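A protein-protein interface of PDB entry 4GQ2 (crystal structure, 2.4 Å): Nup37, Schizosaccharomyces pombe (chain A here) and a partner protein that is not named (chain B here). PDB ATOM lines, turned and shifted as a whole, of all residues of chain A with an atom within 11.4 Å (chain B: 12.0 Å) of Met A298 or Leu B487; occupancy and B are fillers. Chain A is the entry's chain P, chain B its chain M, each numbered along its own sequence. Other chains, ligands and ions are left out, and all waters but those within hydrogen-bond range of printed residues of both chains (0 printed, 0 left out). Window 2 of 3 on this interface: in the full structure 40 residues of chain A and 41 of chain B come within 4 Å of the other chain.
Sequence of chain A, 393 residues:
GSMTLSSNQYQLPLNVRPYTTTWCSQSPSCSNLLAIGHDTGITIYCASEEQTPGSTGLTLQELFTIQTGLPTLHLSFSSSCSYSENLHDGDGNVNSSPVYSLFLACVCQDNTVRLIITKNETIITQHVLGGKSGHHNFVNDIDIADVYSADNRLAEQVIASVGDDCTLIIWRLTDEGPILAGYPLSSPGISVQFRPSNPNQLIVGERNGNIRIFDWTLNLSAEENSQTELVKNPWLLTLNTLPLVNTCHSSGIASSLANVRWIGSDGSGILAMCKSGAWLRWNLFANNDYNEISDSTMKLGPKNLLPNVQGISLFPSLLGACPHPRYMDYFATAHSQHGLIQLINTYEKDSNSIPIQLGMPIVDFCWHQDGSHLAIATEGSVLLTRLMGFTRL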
ATOM      1  N   ARG A 195     -16.323   7.402   2.160  1.00  0.00           N
ATOM      2  CA  ARG A 195     -15.832   6.501   1.123  1.00  0.00           C
ATOM      3  C   ARG A 195     -16.929   6.209   0.105  1.00  0.00           C
ATOM      4  O   ARG A 195     -17.948   5.602   0.453  1.00  0.00           O
ATOM      5  CB  ARG A 195     -15.342   5.190   1.729  1.00  0.00           C
ATOM      6  CG  ARG A 195     -14.490   4.371   0.779  1.00  0.00           C
ATOM      7  CD  ARG A 195     -14.039   3.071   1.410  1.00  0.00           C
ATOM      8  NE  ARG A 195     -13.499   2.192   0.382  1.00  0.00           N
ATOM      9  CZ  ARG A 195     -13.465   0.866   0.461  1.00  0.00           C
ATOM     10  NH1 ARG A 195     -13.931   0.234   1.532  1.00  0.00           N
ATOM     11  NH2 ARG A 195     -12.956   0.172  -0.542  1.00  0.00           N
ATOM     12  N   ASN A 198     -19.082   3.058  -0.084  1.00  0.00           N
ATOM     13  CA  ASN A 198     -18.982   2.459   1.248  1.00  0.00           C
ATOM     14  C   ASN A 198     -19.213   3.520   2.324  1.00  0.00           C
ATOM     15  O   ASN A 198     -18.268   3.950   2.984  1.00  0.00           O
ATOM     16  CB  ASN A 198     -17.620   1.786   1.454  1.00  0.00           C
ATOM     17  CG  ASN A 198     -17.282   0.779   0.368  1.00  0.00           C
ATOM     18  OD1 ASN A 198     -17.136   1.130  -0.804  1.00  0.00           O
ATOM     19  ND2 ASN A 198     -17.127  -0.478   0.762  1.00  0.00           N
ATOM     20  N   GLN A 201     -17.546   3.979   6.068  1.00  0.00           N
ATOM     21  CA  GLN A 201     -16.164   4.403   6.271  1.00  0.00           C
ATOM     22  C   GLN A 201     -15.994   5.854   5.839  1.00  0.00           C
ATOM     23  O   GLN A 201     -16.641   6.316   4.893  1.00  0.00           O
ATOM     24  CB  GLN A 201     -15.180   3.506   5.506  1.00  0.00           C
ATOM     25  CG  GLN A 201     -15.151   2.039   5.949  1.00  0.00           C
ATOM     26  CD  GLN A 201     -14.010   1.247   5.320  1.00  0.00           C
ATOM     27  OE1 GLN A 201     -13.376   1.692   4.362  1.00  0.00           O
ATOM     28  NE2 GLN A 201     -13.741   0.066   5.862  1.00  0.00           N
ATOM     29  N   ASN A 283      -2.932   2.951  -3.108  1.00  0.00           N
ATOM     30  CA  ASN A 283      -3.923   2.060  -3.713  1.00  0.00           C
ATOM     31  C   ASN A 283      -4.297   0.986  -2.709  1.00  0.00           C
ATOM     32  O   ASN A 283      -3.771  -0.124  -2.745  1.00  0.00           O
ATOM     33  CB  ASN A 283      -3.384   1.425  -4.991  1.00  0.00           C
ATOM     34  CG  ASN A 283      -3.057   2.444  -6.055  1.00  0.00           C
ATOM     35  OD1 ASN A 283      -3.822   3.382  -6.302  1.00  0.00           O
ATOM     36  ND2 ASN A 283      -1.910   2.266  -6.699  1.00  0.00           N
ATOM     37  N   LEU A 284      -5.200   1.340  -1.805  1.00  0.00           N
ATOM     38  CA  LEU A 284      -5.520   0.504  -0.661  1.00  0.00           C
ATOM     39  C   LEU A 284      -6.429  -0.656  -1.002  1.00  0.00           C
ATOM     40  O   LEU A 284      -6.168  -1.785  -0.598  1.00  0.00           O
ATOM     41  CB  LEU A 284      -6.184   1.333   0.438  1.00  0.00           C
ATOM     42  CG  LEU A 284      -5.430   1.585   1.732  1.00  0.00           C
ATOM     43  CD1 LEU A 284      -6.461   1.990   2.766  1.00  0.00           C
ATOM     44  CD2 LEU A 284      -4.688   0.342   2.195  1.00  0.00           C
ATOM     45  N   PHE A 285      -7.502  -0.364  -1.732  1.00  0.00           N
ATOM     46  CA  PHE A 285      -8.554  -1.337  -1.973  1.00  0.00           C
ATOM     47  C   PHE A 285      -8.729  -1.652  -3.459  1.00  0.00           C
ATOM     48  O   PHE A 285      -8.230  -0.924  -4.323  1.00  0.00           O
ATOM     49  CB  PHE A 285      -9.877  -0.835  -1.381  1.00  0.00           C
ATOM     50  CG  PHE A 285      -9.819  -0.532   0.094  1.00  0.00           C
ATOM     51  CD1 PHE A 285      -9.603  -1.544   1.028  1.00  0.00           C
ATOM     52  CD2 PHE A 285     -10.010   0.769   0.557  1.00  0.00           C
ATOM     53  CE1 PHE A 285      -9.568  -1.265   2.389  1.00  0.00           C
ATOM     54  CE2 PHE A 285      -9.979   1.053   1.916  1.00  0.00           C
ATOM     55  CZ  PHE A 285      -9.754   0.036   2.835  1.00  0.00           C
ATOM     56  N   ALA A 286      -9.438  -2.739  -3.745  1.00  0.00           N
ATOM     57  CA  ALA A 286      -9.739  -3.138  -5.120  1.00  0.00           C
ATOM     58  C   ALA A 286     -10.668  -2.139  -5.794  1.00  0.00           C
ATOM     59  O   ALA A 286     -11.660  -1.713  -5.199  1.00  0.00           O
ATOM     60  CB  ALA A 286     -10.358  -4.529  -5.144  1.00  0.00           C
ATOM     61  N   ASN A 287     -10.347  -1.759  -7.029  1.00  0.00           N
ATOM     62  CA  ASN A 287     -11.242  -0.908  -7.809  1.00  0.00           C
ATOM     63  C   ASN A 287     -12.413  -1.725  -8.355  1.00  0.00           C
ATOM     64  O   ASN A 287     -12.435  -2.106  -9.531  1.00  0.00           O
ATOM     65  CB  ASN A 287     -10.494  -0.169  -8.927  1.00  0.00           C
ATOM     66  CG  ASN A 287     -11.258   1.045  -9.433  1.00  0.00           C
ATOM     67  OD1 ASN A 287     -12.059   1.644  -8.707  1.00  0.00           O
ATOM     68  ND2 ASN A 287     -11.012   1.416 -10.681  1.00  0.00           N
ATOM     69  N   ASN A 288     -13.380  -1.988  -7.476  1.00  0.00           N
ATOM     70  CA  ASN A 288     -14.467  -2.924  -7.747  1.00  0.00           C
ATOM     71  C   ASN A 288     -15.577  -2.833  -6.696  1.00  0.00           C
ATOM     72  O   ASN A 288     -15.301  -2.599  -5.516  1.00  0.00           O
ATOM     73  CB  ASN A 288     -13.913  -4.352  -7.798  1.00  0.00           C
ATOM     74  CG  ASN A 288     -14.938  -5.357  -8.269  1.00  0.00           C
ATOM     75  OD1 ASN A 288     -15.223  -5.464  -9.463  1.00  0.00           O
ATOM     76  ND2 ASN A 288     -15.498  -6.104  -7.330  1.00  0.00           N
ATOM     77  N   ASP A 289     -16.820  -3.040  -7.138  1.00  0.00           N
ATOM     78  CA  ASP A 289     -18.027  -2.947  -6.296  1.00  0.00           C
ATOM     79  C   ASP A 289     -18.035  -3.854  -5.066  1.00  0.00           C
ATOM     80  O   ASP A 289     -18.551  -3.469  -4.016  1.00  0.00           O
ATOM     81  CB  ASP A 289     -19.284  -3.255  -7.125  1.00  0.00           C
ATOM     82  CG  ASP A 289     -19.600  -2.180  -8.153  1.00  0.00           C
ATOM     83  OD1 ASP A 289     -19.459  -0.977  -7.841  1.00  0.00           O
ATOM     84  OD2 ASP A 289     -20.012  -2.546  -9.276  1.00  0.00           O
ATOM     85  N   TYR A 290     -17.475  -5.054  -5.207  1.00  0.00           N
ATOM     86  CA  TYR A 290     -17.543  -6.081  -4.167  1.00  0.00           C
ATOM     87  C   TYR A 290     -16.273  -6.135  -3.314  1.00  0.00           C
ATOM     88  O   TYR A 290     -16.303  -5.793  -2.126  1.00  0.00           O
ATOM     89  CB  TYR A 290     -17.828  -7.453  -4.801  1.00  0.00           C
ATOM     90  CG  TYR A 290     -18.285  -8.533  -3.838  1.00  0.00           C
ATOM     91  CD1 TYR A 290     -17.375  -9.200  -3.013  1.00  0.00           C
ATOM     92  CD2 TYR A 290     -19.630  -8.907  -3.769  1.00  0.00           C
ATOM     93  CE1 TYR A 290     -17.792 -10.189  -2.133  1.00  0.00           C
ATOM     94  CE2 TYR A 290     -20.057  -9.901  -2.898  1.00  0.00           C
ATOM     95  CZ  TYR A 290     -19.136 -10.540  -2.083  1.00  0.00           C
ATOM     96  OH  TYR A 290     -19.551 -11.528  -1.218  1.00  0.00           O
ATOM     97  N   ASN A 291     -15.168  -6.560  -3.930  1.00  0.00           N
ATOM     98  CA  ASN A 291     -13.903  -6.814  -3.231  1.00  0.00           C
ATOM     99  C   ASN A 291     -13.286  -5.575  -2.590  1.00  0.00           C
ATOM    100  O   ASN A 291     -13.237  -4.511  -3.210  1.00  0.00           O
ATOM    101  CB  ASN A 291     -12.878  -7.444  -4.184  1.00  0.00           C
ATOM    102  CG  ASN A 291     -13.362  -8.746  -4.800  1.00  0.00           C
ATOM    103  OD1 ASN A 291     -14.195  -9.460  -4.231  1.00  0.00           O
ATOM    104  ND2 ASN A 291     -12.830  -9.066  -5.972  1.00  0.00           N
ATOM    105  N   GLU A 292     -12.818  -5.726  -1.352  1.00  0.00           N
ATOM    106  CA  GLU A 292     -12.037  -4.683  -0.683  1.00  0.00           C
ATOM    107  C   GLU A 292     -10.540  -4.845  -0.954  1.00  0.00           C
ATOM    108  O   GLU A 292      -9.863  -3.878  -1.284  1.00  0.00           O
ATOM    109  CB  GLU A 292     -12.333  -4.637   0.822  1.00  0.00           C
ATOM    110  CG  GLU A 292     -13.318  -3.543   1.234  1.00  0.00           C
ATOM    111  CD  GLU A 292     -14.710  -3.721   0.644  1.00  0.00           C
ATOM    112  OE1 GLU A 292     -15.209  -4.868   0.610  1.00  0.00           O
ATOM    113  OE2 GLU A 292     -15.312  -2.710   0.220  1.00  0.00           O
ATOM    114  N   ILE A 293     -10.034  -6.068  -0.829  1.00  0.00           N
ATOM    115  CA  ILE A 293      -8.637  -6.377  -1.154  1.00  0.00           C
ATOM    116  C   ILE A 293      -8.395  -6.317  -2.664  1.00  0.00           C
ATOM    117  O   ILE A 293      -9.073  -7.001  -3.437  1.00  0.00           O
ATOM    118  CB  ILE A 293      -8.240  -7.756  -0.586  1.00  0.00           C
ATOM    119  CG1 ILE A 293      -8.169  -7.674   0.938  1.00  0.00           C
ATOM    120  CG2 ILE A 293      -6.913  -8.245  -1.160  1.00  0.00           C
ATOM    121  CD1 ILE A 293      -8.968  -8.750   1.629  1.00  0.00           C
ATOM    122  N   SER A 294      -7.434  -5.486  -3.072  1.00  0.00           N
ATOM    123  CA  SER A 294      -7.071  -5.333  -4.484  1.00  0.00           C
ATOM    124  C   SER A 294      -6.408  -6.589  -5.042  1.00  0.00           C
ATOM    125  O   SER A 294      -5.582  -7.216  -4.370  1.00  0.00           O
ATOM    126  CB  SER A 294      -6.167  -4.109  -4.697  1.00  0.00           C
ATOM    127  OG  SER A 294      -4.802  -4.415  -4.457  1.00  0.00           O
ATOM    128  N   ASP A 295      -6.779  -6.944  -6.273  1.00  0.00           N
ATOM    129  CA  ASP A 295      -6.191  -8.082  -6.984  1.00  0.00           C
ATOM    130  C   ASP A 295      -4.661  -8.064  -6.896  1.00  0.00           C
ATOM    131  O   ASP A 295      -4.026  -9.118  -6.805  1.00  0.00           O
ATOM    132  CB  ASP A 295      -6.670  -8.102  -8.444  1.00  0.00           C
ATOM    133  CG  ASP A 295      -5.881  -9.070  -9.317  1.00  0.00           C
ATOM    134  OD1 ASP A 295      -4.837  -8.656  -9.868  1.00  0.00           O
ATOM    135  OD2 ASP A 295      -6.312 -10.234  -9.464  1.00  0.00           O
ATOM    136  N   SER A 296      -4.090  -6.860  -6.903  1.00  0.00           N
ATOM    137  CA  SER A 296      -2.646  -6.658  -6.787  1.00  0.00           C
ATOM    138  C   SER A 296      -2.062  -7.223  -5.488  1.00  0.00           C
ATOM    139  O   SER A 296      -0.984  -7.815  -5.504  1.00  0.00           O
ATOM    140  CB  SER A 296      -2.302  -5.172  -6.922  1.00  0.00           C
ATOM    141  OG  SER A 296      -0.899  -4.972  -6.903  1.00  0.00           O
ATOM    142  N   THR A 297      -2.780  -7.044  -4.378  1.00  0.00           N
ATOM    143  CA  THR A 297      -2.367  -7.570  -3.069  1.00  0.00           C
ATOM    144  C   THR A 297      -2.421  -9.102  -3.033  1.00  0.00           C
ATOM    145  O   THR A 297      -1.664  -9.744  -2.298  1.00  0.00           O
ATOM    146  CB  THR A 297      -3.247  -6.996  -1.927  1.00  0.00           C
ATOM    147  OG1 THR A 297      -3.269  -5.568  -2.008  1.00  0.00           O
ATOM    148  CG2 THR A 297      -2.725  -7.404  -0.548  1.00  0.00           C
ATOM    149  N   MET A 298      -3.301  -9.679  -3.848  1.00  0.00           N
ATOM    150  CA  MET A 298      -3.620 -11.101  -3.751  1.00  0.00           C
ATOM    151  C   MET A 298      -2.480 -12.070  -4.094  1.00  0.00           C
ATOM    152  O   MET A 298      -2.429 -13.171  -3.542  1.00  0.00           O
ATOM    153  CB  MET A 298      -4.884 -11.431  -4.552  1.00  0.00           C
ATOM    154  CG  MET A 298      -5.786 -12.466  -3.895  1.00  0.00           C
ATOM    155  SD  MET A 298      -6.245 -12.043  -2.200  1.00  0.00           S
ATOM    156  CE  MET A 298      -4.998 -12.911  -1.247  1.00  0.00           C
ATOM    157  N   LYS A 299      -1.569 -11.665  -4.980  1.00  0.00           N
ATOM    158  CA  LYS A 299      -0.468 -12.552  -5.403  1.00  0.00           C
ATOM    159  C   LYS A 299       0.967 -12.088  -5.122  1.00  0.00           C
ATOM    160  O   LYS A 299       1.853 -12.925  -4.924  1.00  0.00           O
ATOM    161  CB  LYS A 299      -0.621 -13.016  -6.864  1.00  0.00           C
ATOM    162  CG  LYS A 299      -1.641 -12.260  -7.700  1.00  0.00           C
ATOM    163  CD  LYS A 299      -1.099 -10.944  -8.225  1.00  0.00           C
ATOM    164  CE  LYS A 299      -2.112 -10.304  -9.154  1.00  0.00           C
ATOM    165  NZ  LYS A 299      -1.707  -8.947  -9.600  1.00  0.00           N
ATOM    166  N   LEU A 300       1.205 -10.776  -5.109  1.00  0.00           N
ATOM    167  CA  LEU A 300       2.542 -10.254  -4.778  1.00  0.00           C
ATOM    168  C   LEU A 300       2.776 -10.135  -3.265  1.00  0.00           C
ATOM    169  O   LEU A 300       3.849  -9.712  -2.822  1.00  0.00           O
ATOM    170  CB  LEU A 300       2.843  -8.934  -5.513  1.00  0.00           C
ATOM    171  CG  LEU A 300       1.988  -7.676  -5.319  1.00  0.00           C
ATOM    172  CD1 LEU A 300       2.339  -6.918  -4.047  1.00  0.00           C
ATOM    173  CD2 LEU A 300       2.137  -6.760  -6.520  1.00  0.00           C
ATOM    174  N   GLY A 301       1.763 -10.518  -2.486  1.00  0.00           N
ATOM    175  CA  GLY A 301       1.864 -10.590  -1.031  1.00  0.00           C
ATOM    176  C   GLY A 301       1.389  -9.340  -0.313  1.00  0.00           C
ATOM    177  O   GLY A 301       1.126  -8.316  -0.953  1.00  0.00           O
ATOM    178  N   PRO A 302       1.258  -9.419   1.026  1.00  0.00           N
ATOM    179  CA  PRO A 302       0.958  -8.241   1.836  1.00  0.00           C
ATOM    180  C   PRO A 302       2.010  -7.149   1.651  1.00  0.00           C
ATOM    181  O   PRO A 302       3.217  -7.428   1.680  1.00  0.00           O
ATOM    182  CB  PRO A 302       0.986  -8.776   3.277  1.00  0.00           C
ATOM    183  CG  PRO A 302       1.580 -10.145   3.201  1.00  0.00           C
ATOM    184  CD  PRO A 302       1.250 -10.650   1.833  1.00  0.00           C
ATOM    185  N   LYS A 303       1.546  -5.922   1.438  1.00  0.00           N
ATOM    186  CA  LYS A 303       2.445  -4.785   1.298  1.00  0.00           C
ATOM    187  C   LYS A 303       2.428  -3.888   2.530  1.00  0.00           C
ATOM    188  O   LYS A 303       1.542  -3.981   3.384  1.00  0.00           O
ATOM    189  CB  LYS A 303       2.118  -3.967   0.040  1.00  0.00           C
ATOM    190  CG  LYS A 303       2.564  -4.584  -1.283  1.00  0.00           C
ATOM    191  CD  LYS A 303       4.080  -4.676  -1.441  1.00  0.00           C
ATOM    192  CE  LYS A 303       4.597  -6.080  -1.143  1.00  0.00           C
ATOM    193  NZ  LYS A 303       6.003  -6.287  -1.587  1.00  0.00           N
ATOM    194  N   GLN B 480       3.828  -5.040   7.354  1.00  0.00           N
ATOM    195  CA  GLN B 480       2.902  -5.356   6.277  1.00  0.00           C
ATOM    196  C   GLN B 480       1.489  -5.553   6.797  1.00  0.00           C
ATOM    197  O   GLN B 480       1.282  -6.172   7.837  1.00  0.00           O
ATOM    198  CB  GLN B 480       3.371  -6.604   5.524  1.00  0.00           C
ATOM    199  CG  GLN B 480       4.736  -6.449   4.866  1.00  0.00           C
ATOM    200  CD  GLN B 480       5.206  -7.707   4.156  1.00  0.00           C
ATOM    201  OE1 GLN B 480       4.542  -8.750   4.191  1.00  0.00           O
ATOM    202  NE2 GLN B 480       6.360  -7.614   3.504  1.00  0.00           N
ATOM    203  N   ILE B 481       0.526  -5.001   6.065  1.00  0.00           N
ATOM    204  CA  ILE B 481      -0.882  -5.145   6.385  1.00  0.00           C
ATOM    205  C   ILE B 481      -1.464  -6.350   5.641  1.00  0.00           C
ATOM    206  O   ILE B 481      -1.229  -6.535   4.440  1.00  0.00           O
ATOM    207  CB  ILE B 481      -1.673  -3.848   6.084  1.00  0.00           C
ATOM    208  CG1 ILE B 481      -3.101  -3.948   6.628  1.00  0.00           C
ATOM    209  CG2 ILE B 481      -1.656  -3.515   4.594  1.00  0.00           C
ATOM    210  CD1 ILE B 481      -3.864  -2.636   6.624  1.00  0.00           C
ATOM    211  N   GLU B 482      -2.220  -7.166   6.366  1.00  0.00           N
ATOM    212  CA  GLU B 482      -2.776  -8.392   5.808  1.00  0.00           C
ATOM    213  C   GLU B 482      -4.292  -8.387   5.701  1.00  0.00           C
ATOM    214  O   GLU B 482      -4.980  -7.843   6.569  1.00  0.00           O
ATOM    215  CB  GLU B 482      -2.312  -9.603   6.616  1.00  0.00           C
ATOM    216  CG  GLU B 482      -0.971 -10.132   6.145  1.00  0.00           C
ATOM    217  CD  GLU B 482      -0.279 -10.986   7.177  1.00  0.00           C
ATOM    218  OE1 GLU B 482      -0.123 -10.520   8.329  1.00  0.00           O
ATOM    219  OE2 GLU B 482       0.122 -12.118   6.826  1.00  0.00           O
ATOM    220  N   PRO B 483      -4.813  -8.985   4.617  1.00  0.00           N
ATOM    221  CA  PRO B 483      -6.230  -9.308   4.457  1.00  0.00           C
ATOM    222  C   PRO B 483      -6.753 -10.207   5.583  1.00  0.00           C
ATOM    223  O   PRO B 483      -5.981 -10.980   6.157  1.00  0.00           O
ATOM    224  CB  PRO B 483      -6.268 -10.069   3.124  1.00  0.00           C
ATOM    225  CG  PRO B 483      -4.847 -10.383   2.782  1.00  0.00           C
ATOM    226  CD  PRO B 483      -4.055  -9.273   3.389  1.00  0.00           C
ATOM    227  N   ASN B 484      -8.048 -10.091   5.886  1.00  0.00           N
ATOM    228  CA  ASN B 484      -8.722 -10.889   6.921  1.00  0.00           C
ATOM    229  C   ASN B 484     -10.226 -10.586   6.928  1.00  0.00           C
ATOM    230  O   ASN B 484     -10.624  -9.444   6.676  1.00  0.00           O
ATOM    231  CB  ASN B 484      -8.131 -10.587   8.306  1.00  0.00           C
ATOM    232  CG  ASN B 484      -8.289 -11.739   9.286  1.00  0.00           C
ATOM    233  OD1 ASN B 484      -8.985 -11.618  10.296  1.00  0.00           O
ATOM    234  ND2 ASN B 484      -7.640 -12.864   8.994  1.00  0.00           N
ATOM    235  N   SER B 485     -11.075 -11.581   7.203  1.00  0.00           N
ATOM    236  CA  SER B 485     -10.690 -12.978   7.431  1.00  0.00           C
ATOM    237  C   SER B 485     -11.197 -13.838   6.282  1.00  0.00           C
ATOM    238  O   SER B 485     -10.505 -14.741   5.799  1.00  0.00           O
ATOM    239  CB  SER B 485     -11.272 -13.483   8.751  1.00  0.00           C
ATOM    240  OG  SER B 485     -10.827 -14.798   9.025  1.00  0.00           O
ATOM    241  N   ASP B 486     -12.426 -13.543   5.868  1.00  0.00           N
ATOM    242  CA  ASP B 486     -13.025 -14.104   4.670  1.00  0.00           C
ATOM    243  C   ASP B 486     -12.684 -13.223   3.462  1.00  0.00           C
ATOM    244  O   ASP B 486     -13.468 -13.121   2.512  1.00  0.00           O
ATOM    245  CB  ASP B 486     -14.544 -14.238   4.856  1.00  0.00           C
ATOM    246  CG  ASP B 486     -15.178 -13.015   5.529  1.00  0.00           C
ATOM    247  OD1 ASP B 486     -14.467 -12.240   6.206  1.00  0.00           O
ATOM    248  OD2 ASP B 486     -16.404 -12.836   5.384  1.00  0.00           O
ATOM    249  N   LEU B 487     -11.505 -12.598   3.519  1.00  0.00           N
ATOM    250  CA  LEU B 487     -10.989 -11.706   2.473  1.00  0.00           C
ATOM    251  C   LEU B 487     -11.947 -10.549   2.171  1.00  0.00           C
ATOM    252  O   LEU B 487     -12.203 -10.213   1.013  1.00  0.00           O
ATOM    253  CB  LEU B 487     -10.629 -12.494   1.199  1.00  0.00           C
ATOM    254  CG  LEU B 487      -9.367 -13.378   1.125  1.00  0.00           C
ATOM    255  CD1 LEU B 487      -8.106 -12.532   1.003  1.00  0.00           C
ATOM    256  CD2 LEU B 487      -9.233 -14.386   2.263  1.00  0.00           C
ATOM    257  N   THR B 488     -12.459  -9.938   3.236  1.00  0.00           N
ATOM    258  CA  THR B 488     -13.473  -8.889   3.132  1.00  0.00           C
ATOM    259  C   THR B 488     -12.986  -7.558   3.716  1.00  0.00           C
ATOM    260  O   THR B 488     -13.786  -6.686   4.068  1.00  0.00           O
ATOM    261  CB  THR B 488     -14.787  -9.320   3.822  1.00  0.00           C
ATOM    262  OG1 THR B 488     -14.501  -9.801   5.143  1.00  0.00           O
ATOM    263  CG2 THR B 488     -15.485 -10.419   3.019  1.00  0.00           C
ATOM    264  N   GLY B 489     -11.666  -7.412   3.799  1.00  0.00           N
ATOM    265  CA  GLY B 489     -11.024  -6.233   4.379  1.00  0.00           C
ATOM    266  C   GLY B 489      -9.669  -6.615   4.940  1.00  0.00           C
ATOM    267  O   GLY B 489      -9.259  -7.776   4.850  1.00  0.00           O
ATOM    268  N   TYR B 490      -8.967  -5.647   5.520  1.00  0.00           N
ATOM    269  CA  TYR B 490      -7.671  -5.927   6.129  1.00  0.00           C
ATOM    270  C   TYR B 490      -7.802  -6.244   7.613  1.00  0.00           C
ATOM    271  O   TYR B 490      -8.787  -5.876   8.254  1.00  0.00           O
ATOM    272  CB  TYR B 490      -6.709  -4.759   5.933  1.00  0.00           C
ATOM    273  CG  TYR B 490      -6.335  -4.477   4.494  1.00  0.00           C
ATOM    274  CD1 TYR B 490      -5.311  -5.188   3.869  1.00  0.00           C
ATOM    275  CD2 TYR B 490      -6.984  -3.484   3.766  1.00  0.00           C
ATOM    276  CE1 TYR B 490      -4.954  -4.930   2.554  1.00  0.00           C
ATOM    277  CE2 TYR B 490      -6.636  -3.221   2.448  1.00  0.00           C
ATOM    278  CZ  TYR B 490      -5.620  -3.946   1.851  1.00  0.00           C
ATOM    279  OH  TYR B 490      -5.256  -3.691   0.553  1.00  0.00           O
ATOM    280  N   ASP B 491      -6.806  -6.950   8.142  1.00  0.00           N
ATOM    281  CA  ASP B 491      -6.692  -7.199   9.573  1.00  0.00           C
ATOM    282  C   ASP B 491      -6.016  -5.983  10.199  1.00  0.00           C
ATOM    283  O   ASP B 491      -4.807  -5.974  10.436  1.00  0.00           O
ATOM    284  CB  ASP B 491      -5.879  -8.476   9.843  1.00  0.00           C
ATOM    285  CG  ASP B 491      -5.971  -8.946  11.289  1.00  0.00           C
ATOM    286  OD1 ASP B 491      -6.479  -8.194  12.147  1.00  0.00           O
ATOM    287  OD2 ASP B 491      -5.523 -10.077  11.575  1.00  0.00           O
ATOM    288  N   TYR B 492      -6.816  -4.951  10.437  1.00  0.00           N
ATOM    289  CA  TYR B 492      -6.356  -3.703  11.030  1.00  0.00           C
ATOM    290  C   TYR B 492      -5.758  -3.905  12.418  1.00  0.00           C
ATOM    291  O   TYR B 492      -4.756  -3.276  12.762  1.00  0.00           O
ATOM    292  CB  TYR B 492      -7.516  -2.709  11.092  1.00  0.00           C
ATOM    293  CG  TYR B 492      -8.082  -2.370   9.733  1.00  0.00           C
ATOM    294  CD1 TYR B 492      -7.364  -1.569   8.839  1.00  0.00           C
ATOM    295  CD2 TYR B 492      -9.336  -2.839   9.336  1.00  0.00           C
ATOM    296  CE1 TYR B 492      -7.876  -1.251   7.591  1.00  0.00           C
ATOM    297  CE2 TYR B 492      -9.859  -2.522   8.088  1.00  0.00           C
ATOM    298  CZ  TYR B 492      -9.124  -1.727   7.219  1.00  0.00           C
ATOM    299  OH  TYR B 492      -9.626  -1.400   5.973  1.00  0.00           O
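The side-chain amide oxygen of Gln B480 lies close to the backbone carbonyl oxygen of Pro A302, at 3.1 Å.
The backbone NH (N) of Ile B481 sits at hydrogen-bond distance from the backbone carbonyl oxygen (O) of Lys A303 (3.0 Å).
O of Leu A284 is in hydrogen-bond range of OH of Tyr B490 (2.4 Å).
The backbone carbonyl oxygen of Glu B482 lies within hydrogen-bond range of the backbone NH of Asp B491 (2.6 Å).
The backbone NH of Asn B484 sits at hydrogen-bond distance from the backbone carbonyl oxygen of Gly B489, at 2.8 Å.
The side-chain hydroxyl (OG1) of Thr A297 sits at hydrogen-bond distance from the side-chain hydroxyl (OG) of Ser A294 (3.1 Å).
Among the printed residues, pairs that only touch across the chains: Ile A293 with Pro B483 (3.4 Å), Pro A302 with Ile B481 (3.4 Å), Ile A293 with Gly B489 (3.4 Å), Phe A285 with Tyr B492 (3.5 Å), Lys A303 with Gln B480 (3.5 Å), Ile A293 with Leu B487 (3.5 Å), Phe A285 with Tyr B490 (3.5 Å), Pro A302 with Glu B482 (3.7 Å), Met A298 with Leu B487 (3.7 Å) and Thr A297 with Tyr B490 (3.7 Å).
Of the printed residues of chain B, Leu A284 touches Tyr B490 (2.4 Å).
Asn A291 touches none of the printed residues of chain B.
Ile A293 touches three residues of chain B.
Asp A295 touches none of the printed residues of chain B.
No residue of chain B comes within 4 Å of Ser A296.
Met A298 touches just one residue of chain B: Leu B487 (3.7 Å).
No residue of chain B comes within 4 Å of Lys A299.
Leu A300 touches none of the printed residues of chain B.
No residue of chain B comes within 4 Å of Gly A301.
Printed residues of chain B within 4 Å of Lys A303: Gln B480 (3.5 Å) and Ile B481 (3.0 Å).
Of the printed residues of chain A, Glu B482 touches Pro A302 (3.7 Å).
No residue of chain A comes within 4 Å of Asp B486.
Of chain A, only Ile A293 and Met A298 come within 4 Å of Leu B487.
Gly B489 touches just one residue of chain A: Ile A293 (3.4 Å).
Of the printed residues of chain A, Tyr B490 touches Leu A284, Phe A285 and Thr A297.
Of the printed residues of chain A, Tyr B492 touches Phe A285.
The nearest residue of chain A that does not touch Leu B487 is Glu A292 (5.1 Å).
The nearest printed residue of chain A that does not touch Tyr B492 is Gln A201 (4.4 Å).
Of the 24 printed residues of chain A, 7 touch a printed residue of chain B.
Along chain A the printed residues that touch a printed residue of chain B span positions 284 to 303.
Along chain B the printed residues that touch a printed residue of chain A span positions 480 to 492.
Among the printed residues, 13 pairs touch across the chains.
Among the printed residues, no Asp or Glu carboxylate lies within 4 Å of a Lys or Arg side-chain nitrogen of the other chain.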
